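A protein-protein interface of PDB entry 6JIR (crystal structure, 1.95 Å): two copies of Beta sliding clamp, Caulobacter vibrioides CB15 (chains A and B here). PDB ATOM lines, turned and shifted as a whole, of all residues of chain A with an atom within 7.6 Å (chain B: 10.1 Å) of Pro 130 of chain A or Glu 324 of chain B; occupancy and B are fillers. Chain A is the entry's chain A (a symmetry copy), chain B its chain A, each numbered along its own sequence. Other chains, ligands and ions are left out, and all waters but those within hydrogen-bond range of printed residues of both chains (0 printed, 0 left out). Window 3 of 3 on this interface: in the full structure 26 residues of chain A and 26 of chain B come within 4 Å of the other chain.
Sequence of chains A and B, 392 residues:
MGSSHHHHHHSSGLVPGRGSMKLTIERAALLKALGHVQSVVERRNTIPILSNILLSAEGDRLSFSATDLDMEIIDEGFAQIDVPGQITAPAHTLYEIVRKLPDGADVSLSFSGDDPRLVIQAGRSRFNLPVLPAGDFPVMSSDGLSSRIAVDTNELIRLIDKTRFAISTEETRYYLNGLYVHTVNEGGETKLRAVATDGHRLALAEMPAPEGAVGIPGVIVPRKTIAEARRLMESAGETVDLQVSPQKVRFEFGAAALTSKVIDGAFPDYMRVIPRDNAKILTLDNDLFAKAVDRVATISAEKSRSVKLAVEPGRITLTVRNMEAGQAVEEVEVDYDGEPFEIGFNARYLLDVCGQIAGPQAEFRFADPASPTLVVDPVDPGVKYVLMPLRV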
ATOM      1  N   ASN A  52     -14.584  -7.832  13.003  1.00  0.00           N
ATOM      2  CA  ASN A  52     -13.579  -8.697  13.574  1.00  0.00           C
ATOM      3  C   ASN A  52     -14.101 -10.105  13.872  1.00  0.00           C
ATOM      4  O   ASN A  52     -15.305 -10.333  14.054  1.00  0.00           O
ATOM      5  CB  ASN A  52     -13.028  -8.098  14.885  1.00  0.00           C
ATOM      6  CG  ASN A  52     -12.058  -6.961  14.655  1.00  0.00           C
ATOM      7  OD1 ASN A  52     -11.874  -6.470  13.531  1.00  0.00           O
ATOM      8  ND2 ASN A  52     -11.397  -6.548  15.718  1.00  0.00           N
ATOM      9  N   ILE A  87      -8.926 -12.620  21.946  1.00  0.00           N
ATOM     10  CA  ILE A  87      -8.688 -11.358  21.275  1.00  0.00           C
ATOM     11  C   ILE A  87      -9.558 -11.289  19.996  1.00  0.00           C
ATOM     12  O   ILE A  87     -10.044 -12.327  19.495  1.00  0.00           O
ATOM     13  CB  ILE A  87      -7.175 -11.227  20.982  1.00  0.00           C
ATOM     14  CG1 ILE A  87      -6.722  -9.806  20.644  1.00  0.00           C
ATOM     15  CG2 ILE A  87      -6.752 -12.151  19.851  1.00  0.00           C
ATOM     16  CD1 ILE A  87      -6.929  -8.777  21.736  1.00  0.00           C
ATOM     17  N   THR A  88      -9.738 -10.098  19.474  1.00  0.00           N
ATOM     18  CA  THR A  88     -10.449  -9.921  18.183  1.00  0.00           C
ATOM     19  C   THR A  88      -9.545  -9.252  17.183  1.00  0.00           C
ATOM     20  O   THR A  88      -8.749  -8.372  17.519  1.00  0.00           O
ATOM     21  CB  THR A  88     -11.813  -9.184  18.314  1.00  0.00           C
ATOM     22  OG1 THR A  88     -11.622  -7.775  18.367  1.00  0.00           O
ATOM     23  CG2 THR A  88     -12.604  -9.697  19.535  1.00  0.00           C
ATOM     24  N   ALA A  89      -9.668  -9.656  15.921  1.00  0.00           N
ATOM     25  CA  ALA A  89      -8.839  -9.120  14.858  1.00  0.00           C
ATOM     26  C   ALA A  89      -9.635  -9.100  13.533  1.00  0.00           C
ATOM     27  O   ALA A  89     -10.624  -9.803  13.423  1.00  0.00           O
ATOM     28  CB  ALA A  89      -7.556  -9.911  14.731  1.00  0.00           C
ATOM     29  N   PRO A  90      -9.242  -8.249  12.571  1.00  0.00           N
ATOM     30  CA  PRO A  90     -10.071  -8.068  11.369  1.00  0.00           C
ATOM     31  C   PRO A  90     -10.248  -9.335  10.554  1.00  0.00           C
ATOM     32  O   PRO A  90      -9.231  -9.992  10.210  1.00  0.00           O
ATOM     33  CB  PRO A  90      -9.305  -7.032  10.561  1.00  0.00           C
ATOM     34  CG  PRO A  90      -8.525  -6.280  11.581  1.00  0.00           C
ATOM     35  CD  PRO A  90      -8.137  -7.282  12.607  1.00  0.00           C
ATOM     36  N   THR A  93      -9.167  -9.527   6.508  1.00  0.00           N
ATOM     37  CA  THR A  93      -7.743  -9.468   6.364  1.00  0.00           C
ATOM     38  C   THR A  93      -7.073 -10.732   6.908  1.00  0.00           C
ATOM     39  O   THR A  93      -6.143 -11.243   6.292  1.00  0.00           O
ATOM     40  CB  THR A  93      -7.166  -8.195   7.030  1.00  0.00           C
ATOM     41  OG1 THR A  93      -7.786  -7.077   6.425  1.00  0.00           O
ATOM     42  CG2 THR A  93      -5.644  -8.107   6.859  1.00  0.00           C
ATOM     43  N   PRO A 116      -0.644  -4.205  22.140  1.00  0.00           N
ATOM     44  CA  PRO A 116      -0.627  -5.483  21.451  1.00  0.00           C
ATOM     45  C   PRO A 116      -1.110  -5.369  19.992  1.00  0.00           C
ATOM     46  O   PRO A 116      -1.909  -4.513  19.663  1.00  0.00           O
ATOM     47  CB  PRO A 116      -1.592  -6.329  22.272  1.00  0.00           C
ATOM     48  CG  PRO A 116      -2.597  -5.332  22.786  1.00  0.00           C
ATOM     49  CD  PRO A 116      -1.796  -4.092  23.052  1.00  0.00           C
ATOM     50  N   ARG A 117      -0.527  -6.206  19.146  1.00  0.00           N
ATOM     51  CA  ARG A 117      -1.018  -6.513  17.816  1.00  0.00           C
ATOM     52  C   ARG A 117      -1.128  -8.010  17.754  1.00  0.00           C
ATOM     53  O   ARG A 117      -0.369  -8.693  18.419  1.00  0.00           O
ATOM     54  CB  ARG A 117      -0.005  -6.071  16.760  1.00  0.00           C
ATOM     55  CG  ARG A 117       0.326  -4.592  16.754  1.00  0.00           C
ATOM     56  CD  ARG A 117      -0.709  -3.770  16.013  1.00  0.00           C
ATOM     57  NE  ARG A 117      -0.271  -2.374  15.865  1.00  0.00           N
ATOM     58  CZ  ARG A 117      -0.291  -1.444  16.835  1.00  0.00           C
ATOM     59  NH1 ARG A 117      -0.726  -1.717  18.073  1.00  0.00           N
ATOM     60  NH2 ARG A 117       0.138  -0.220  16.565  1.00  0.00           N
ATOM     61  N   LEU A 118      -2.034  -8.538  16.938  1.00  0.00           N
ATOM     62  CA  LEU A 118      -2.086  -9.968  16.689  1.00  0.00           C
ATOM     63  C   LEU A 118      -0.937 -10.321  15.741  1.00  0.00           C
ATOM     64  O   LEU A 118      -0.845  -9.785  14.627  1.00  0.00           O
ATOM     65  CB  LEU A 118      -3.407 -10.415  16.097  1.00  0.00           C
ATOM     66  CG  LEU A 118      -3.468 -11.892  15.753  1.00  0.00           C
ATOM     67  CD1 LEU A 118      -3.374 -12.778  17.018  1.00  0.00           C
ATOM     68  CD2 LEU A 118      -4.687 -12.256  14.928  1.00  0.00           C
ATOM     69  N   ASN A 128       1.405  -8.352  11.482  1.00  0.00           N
ATOM     70  CA  ASN A 128       0.879  -7.742  12.699  1.00  0.00           C
ATOM     71  C   ASN A 128      -0.456  -7.077  12.315  1.00  0.00           C
ATOM     72  O   ASN A 128      -0.478  -6.243  11.400  1.00  0.00           O
ATOM     73  CB  ASN A 128       1.862  -6.681  13.240  1.00  0.00           C
ATOM     74  CG  ASN A 128       3.191  -7.293  13.733  1.00  0.00           C
ATOM     75  OD1 ASN A 128       3.822  -8.099  13.052  1.00  0.00           O
ATOM     76  ND2 ASN A 128       3.608  -6.913  14.918  1.00  0.00           N
ATOM     77  N   LEU A 129      -1.553  -7.434  12.993  1.00  0.00           N
ATOM     78  CA  LEU A 129      -2.832  -6.771  12.792  1.00  0.00           C
ATOM     79  C   LEU A 129      -3.320  -6.047  14.047  1.00  0.00           C
ATOM     80  O   LEU A 129      -3.089  -6.531  15.167  1.00  0.00           O
ATOM     81  CB  LEU A 129      -3.906  -7.804  12.429  1.00  0.00           C
ATOM     82  CG  LEU A 129      -3.732  -8.591  11.140  1.00  0.00           C
ATOM     83  CD1 LEU A 129      -4.865  -9.577  11.029  1.00  0.00           C
ATOM     84  CD2 LEU A 129      -3.686  -7.664   9.950  1.00  0.00           C
ATOM     85  N   PRO A 130      -4.065  -4.952  13.864  1.00  0.00           N
ATOM     86  CA  PRO A 130      -4.652  -4.274  15.023  1.00  0.00           C
ATOM     87  C   PRO A 130      -5.746  -5.131  15.640  1.00  0.00           C
ATOM     88  O   PRO A 130      -6.452  -5.884  14.925  1.00  0.00           O
ATOM     89  CB  PRO A 130      -5.218  -2.987  14.419  1.00  0.00           C
ATOM     90  CG  PRO A 130      -5.614  -3.406  13.055  1.00  0.00           C
ATOM     91  CD  PRO A 130      -4.522  -4.343  12.604  1.00  0.00           C
ATOM     92  N   VAL A 131      -5.912  -5.007  16.950  1.00  0.00           N
ATOM     93  CA  VAL A 131      -6.843  -5.827  17.692  1.00  0.00           C
ATOM     94  C   VAL A 131      -7.796  -5.003  18.509  1.00  0.00           C
ATOM     95  O   VAL A 131      -7.533  -3.836  18.800  1.00  0.00           O
ATOM     96  CB  VAL A 131      -6.120  -6.822  18.616  1.00  0.00           C
ATOM     97  CG1 VAL A 131      -5.357  -7.838  17.787  1.00  0.00           C
ATOM     98  CG2 VAL A 131      -5.212  -6.107  19.605  1.00  0.00           C
ATOM     99  N   LEU A 132      -8.917  -5.600  18.859  1.00  0.00           N
ATOM    100  CA  LEU A 132      -9.824  -4.988  19.831  1.00  0.00           C
ATOM    101  C   LEU A 132     -10.124  -6.026  20.890  1.00  0.00           C
ATOM    102  O   LEU A 132     -10.104  -7.235  20.607  1.00  0.00           O
ATOM    103  CB  LEU A 132     -11.107  -4.438  19.178  1.00  0.00           C
ATOM    104  CG  LEU A 132     -10.920  -3.350  18.151  1.00  0.00           C
ATOM    105  CD1 LEU A 132     -12.206  -3.161  17.344  1.00  0.00           C
ATOM    106  CD2 LEU A 132     -10.504  -2.055  18.846  1.00  0.00           C
ATOM    107  N   THR B 298      -0.849  -8.818   0.696  1.00  0.00           N
ATOM    108  CA  THR B 298      -2.175  -9.241   1.138  1.00  0.00           C
ATOM    109  C   THR B 298      -2.579  -8.573   2.453  1.00  0.00           C
ATOM    110  O   THR B 298      -3.728  -8.629   2.821  1.00  0.00           O
ATOM    111  CB  THR B 298      -2.245 -10.770   1.239  1.00  0.00           C
ATOM    112  OG1 THR B 298      -2.003 -11.353  -0.061  1.00  0.00           O
ATOM    113  CG2 THR B 298      -3.615 -11.263   1.693  1.00  0.00           C
ATOM    114  N   ILE B 299      -1.640  -7.931   3.152  1.00  0.00           N
ATOM    115  CA  ILE B 299      -1.972  -7.050   4.279  1.00  0.00           C
ATOM    116  C   ILE B 299      -2.895  -5.899   3.862  1.00  0.00           C
ATOM    117  O   ILE B 299      -3.574  -5.345   4.698  1.00  0.00           O
ATOM    118  CB  ILE B 299      -0.697  -6.490   4.982  1.00  0.00           C
ATOM    119  CG1 ILE B 299      -1.000  -5.871   6.361  1.00  0.00           C
ATOM    120  CG2 ILE B 299       0.034  -5.487   4.114  1.00  0.00           C
ATOM    121  CD1 ILE B 299      -1.278  -6.892   7.441  1.00  0.00           C
ATOM    122  N   SER B 300      -2.902  -5.540   2.585  1.00  0.00           N
ATOM    123  CA  SER B 300      -3.619  -4.357   2.097  1.00  0.00           C
ATOM    124  C   SER B 300      -4.579  -4.728   0.969  1.00  0.00           C
ATOM    125  O   SER B 300      -4.269  -5.580   0.145  1.00  0.00           O
ATOM    126  CB  SER B 300      -2.619  -3.290   1.634  1.00  0.00           C
ATOM    127  OG  SER B 300      -3.294  -2.161   1.122  1.00  0.00           O
ATOM    128  N   ALA B 301      -5.762  -4.100   0.986  1.00  0.00           N
ATOM    129  CA  ALA B 301      -6.763  -4.189  -0.087  1.00  0.00           C
ATOM    130  C   ALA B 301      -6.755  -2.960  -1.014  1.00  0.00           C
ATOM    131  O   ALA B 301      -7.610  -2.845  -1.897  1.00  0.00           O
ATOM    132  CB  ALA B 301      -8.154  -4.396   0.507  1.00  0.00           C
ATOM    133  N   GLU B 302      -5.784  -2.059  -0.833  1.00  0.00           N
ATOM    134  CA  GLU B 302      -5.662  -0.856  -1.658  1.00  0.00           C
ATOM    135  C   GLU B 302      -5.324  -1.171  -3.109  1.00  0.00           C
ATOM    136  O   GLU B 302      -4.854  -2.269  -3.428  1.00  0.00           O
ATOM    137  CB  GLU B 302      -4.579   0.065  -1.114  1.00  0.00           C
ATOM    138  CG  GLU B 302      -4.888   0.643   0.253  1.00  0.00           C
ATOM    139  CD  GLU B 302      -3.760   1.514   0.764  1.00  0.00           C
ATOM    140  OE1 GLU B 302      -3.397   1.391   1.956  1.00  0.00           O
ATOM    141  OE2 GLU B 302      -3.232   2.317  -0.035  1.00  0.00           O
ATOM    142  N   VAL B 320       5.297  -4.533   3.619  1.00  0.00           N
ATOM    143  CA  VAL B 320       4.102  -3.810   3.164  1.00  0.00           C
ATOM    144  C   VAL B 320       3.329  -3.359   4.411  1.00  0.00           C
ATOM    145  O   VAL B 320       3.279  -4.070   5.421  1.00  0.00           O
ATOM    146  CB  VAL B 320       3.190  -4.676   2.254  1.00  0.00           C
ATOM    147  CG1 VAL B 320       1.924  -3.924   1.811  1.00  0.00           C
ATOM    148  CG2 VAL B 320       3.949  -5.154   1.002  1.00  0.00           C
ATOM    149  N   ARG B 321       2.759  -2.164   4.326  1.00  0.00           N
ATOM    150  CA  ARG B 321       1.856  -1.629   5.349  1.00  0.00           C
ATOM    151  C   ARG B 321       0.514  -1.268   4.721  1.00  0.00           C
ATOM    152  O   ARG B 321       0.441  -1.008   3.511  1.00  0.00           O
ATOM    153  CB  ARG B 321       2.472  -0.417   6.036  1.00  0.00           C
ATOM    154  CG  ARG B 321       3.614  -0.822   6.936  1.00  0.00           C
ATOM    155  CD  ARG B 321       4.138   0.322   7.789  1.00  0.00           C
ATOM    156  NE  ARG B 321       5.197  -0.163   8.685  1.00  0.00           N
ATOM    157  CZ  ARG B 321       6.454  -0.449   8.325  1.00  0.00           C
ATOM    158  NH1 ARG B 321       7.316  -0.900   9.238  1.00  0.00           N
ATOM    159  NH2 ARG B 321       6.873  -0.293   7.062  1.00  0.00           N
ATOM    160  N   ASN B 322      -0.551  -1.319   5.528  1.00  0.00           N
ATOM    161  CA  ASN B 322      -1.852  -0.777   5.117  1.00  0.00           C
ATOM    162  C   ASN B 322      -2.088   0.521   5.885  1.00  0.00           C
ATOM    163  O   ASN B 322      -1.214   0.956   6.644  1.00  0.00           O
ATOM    164  CB  ASN B 322      -3.009  -1.830   5.213  1.00  0.00           C
ATOM    165  CG  ASN B 322      -3.366  -2.259   6.652  1.00  0.00           C
ATOM    166  OD1 ASN B 322      -3.210  -1.512   7.627  1.00  0.00           O
ATOM    167  ND2 ASN B 322      -3.884  -3.475   6.769  1.00  0.00           N
ATOM    168  N   MET B 323      -3.234   1.154   5.632  1.00  0.00           N
ATOM    169  CA  MET B 323      -3.617   2.421   6.298  1.00  0.00           C
ATOM    170  C   MET B 323      -4.125   2.232   7.746  1.00  0.00           C
ATOM    171  O   MET B 323      -4.215   3.208   8.501  1.00  0.00           O
ATOM    172  CB  MET B 323      -4.694   3.137   5.469  1.00  0.00           C
ATOM    173  N   GLU B 324      -4.446   0.980   8.108  1.00  0.00           N
ATOM    174  CA  GLU B 324      -5.012   0.606   9.416  1.00  0.00           C
ATOM    175  C   GLU B 324      -4.003  -0.129  10.341  1.00  0.00           C
ATOM    176  O   GLU B 324      -4.335  -1.175  10.911  1.00  0.00           O
ATOM    177  CB  GLU B 324      -6.270  -0.282   9.205  1.00  0.00           C
ATOM    178  CG  GLU B 324      -7.461   0.390   8.514  1.00  0.00           C
ATOM    179  CD  GLU B 324      -7.317   0.516   7.000  1.00  0.00           C
ATOM    180  OE1 GLU B 324      -6.632  -0.314   6.358  1.00  0.00           O
ATOM    181  OE2 GLU B 324      -7.908   1.459   6.438  1.00  0.00           O
ATOM    182  N   ALA B 325      -2.784   0.405  10.456  1.00  0.00           N
ATOM    183  CA  ALA B 325      -1.736  -0.095  11.379  1.00  0.00           C
ATOM    184  C   ALA B 325      -1.327  -1.583  11.204  1.00  0.00           C
ATOM    185  O   ALA B 325      -0.765  -2.207  12.116  1.00  0.00           O
ATOM    186  CB  ALA B 325      -2.140   0.170  12.818  1.00  0.00           C
ATOM    187  N   GLY B 326      -1.636  -2.157  10.050  1.00  0.00           N
ATOM    188  CA  GLY B 326      -1.274  -3.528   9.751  1.00  0.00           C
ATOM    189  C   GLY B 326       0.087  -3.504   9.065  1.00  0.00           C
ATOM    190  O   GLY B 326       0.397  -2.576   8.310  1.00  0.00           O
ATOM    191  N   GLN B 327       0.880  -4.520   9.332  1.00  0.00           N
ATOM    192  CA  GLN B 327       2.215  -4.638   8.756  1.00  0.00           C
ATOM    193  C   GLN B 327       2.487  -6.066   8.374  1.00  0.00           C
ATOM    194  O   GLN B 327       2.101  -6.968   9.105  1.00  0.00           O
ATOM    195  CB  GLN B 327       3.254  -4.203   9.784  1.00  0.00           C
ATOM    196  CG  GLN B 327       4.660  -4.150   9.226  1.00  0.00           C
ATOM    197  CD  GLN B 327       5.684  -3.980  10.314  1.00  0.00           C
ATOM    198  OE1 GLN B 327       6.174  -2.885  10.520  1.00  0.00           O
ATOM    199  NE2 GLN B 327       5.997  -5.059  11.029  1.00  0.00           N
ATOM    200  N   ALA B 328       3.189  -6.262   7.252  1.00  0.00           N
ATOM    201  CA  ALA B 328       3.632  -7.595   6.806  1.00  0.00           C
ATOM    202  C   ALA B 328       5.112  -7.547   6.437  1.00  0.00           C
ATOM    203  O   ALA B 328       5.575  -6.577   5.841  1.00  0.00           O
ATOM    204  CB  ALA B 328       2.816  -8.077   5.630  1.00  0.00           C
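O of Ala 325 of chain B touches NE of Arg 117 of chain A, at 3.8 Å.
Asn 128 of chain A touches Gly 326 of chain B.
CD1 of Ile 299 of chain B touches CD2 of Leu 129 of chain A (3.6 Å).
Glu 324 of chain B touches Pro 130 of chain A.
The side-chain amide oxygen (OD1) of Asn 322 of chain B is in hydrogen-bond range of the backbone NH (N) of Gly 326 of chain B, 3.0 Å away.
The backbone carbonyl oxygen (O) of Leu 129 of chain A sits at hydrogen-bond distance from the backbone NH (N) of Leu 118 of chain A, at 2.9 Å.
The backbone NH (N) of Glu 324 of chain B sits at hydrogen-bond distance from the side-chain amide oxygen (OD1) of Asn 322 of chain B (2.8 Å).
N of Ala 325 of chain B lies within hydrogen-bond range of OD1 of Asn 322 of chain B (3.4 Å).
NH1 of Arg 321 of chain B is in hydrogen-bond range of OE1 of Gln 327 of chain B (2.6 Å).
The backbone carbonyl oxygen (O) of Ile 299 of chain B lies within hydrogen-bond range of the side-chain amide nitrogen (ND2) of Asn 322 of chain B.
Of the 14 printed residues of chain A, 4 touch a printed residue of chain B.
Printed residues of chain A that touch a printed residue of chain B: Arg 117, Asn 128, Leu 129 and Pro 130.
Hydrophobic or aromatic side chains of chain A that line the printed part of chain B: Leu 129 and Pro 130.
No position is printed for both chains.
Of the 5 pairs that touch across the chains among the printed residues, none has its exchanged pair printed and touching as well.
Of the printed residues of chain B, Arg 117 of chain A touches Ala 325.
Leu 129 of chain A touches one residue of chain B.
Pro 130 of chain A touches just one residue of chain B: Glu 324 (3.3 Å).
No residue of chain B comes within 4 Å of Val 131 of chain A.
Printed residues of chain A within 4 Å of Ile 299 of chain B: Leu 129.
Glu 324 of chain B touches just one residue of chain A: Pro 130.
Of the printed residues of chain A, Ala 325 of chain B touches Arg 117.
Of the printed residues of chain A, Gly 326 of chain B touches Asn 128 (3.3 Å).
Printed residues of chain A within 4 Å of Gln 327 of chain B: Asn 128.
Ala 328 of chain B touches none of the printed residues of chain A.
The nearest residue of chain A that does not touch Glu 324 of chain B is Leu 129 of chain A (5.9 Å).
The backbone carbonyl oxygen (O) of Gln 327 of chain B sits at hydrogen-bond distance from the backbone NH (N) of Asn 128 of chain A, at 2.8 Å.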
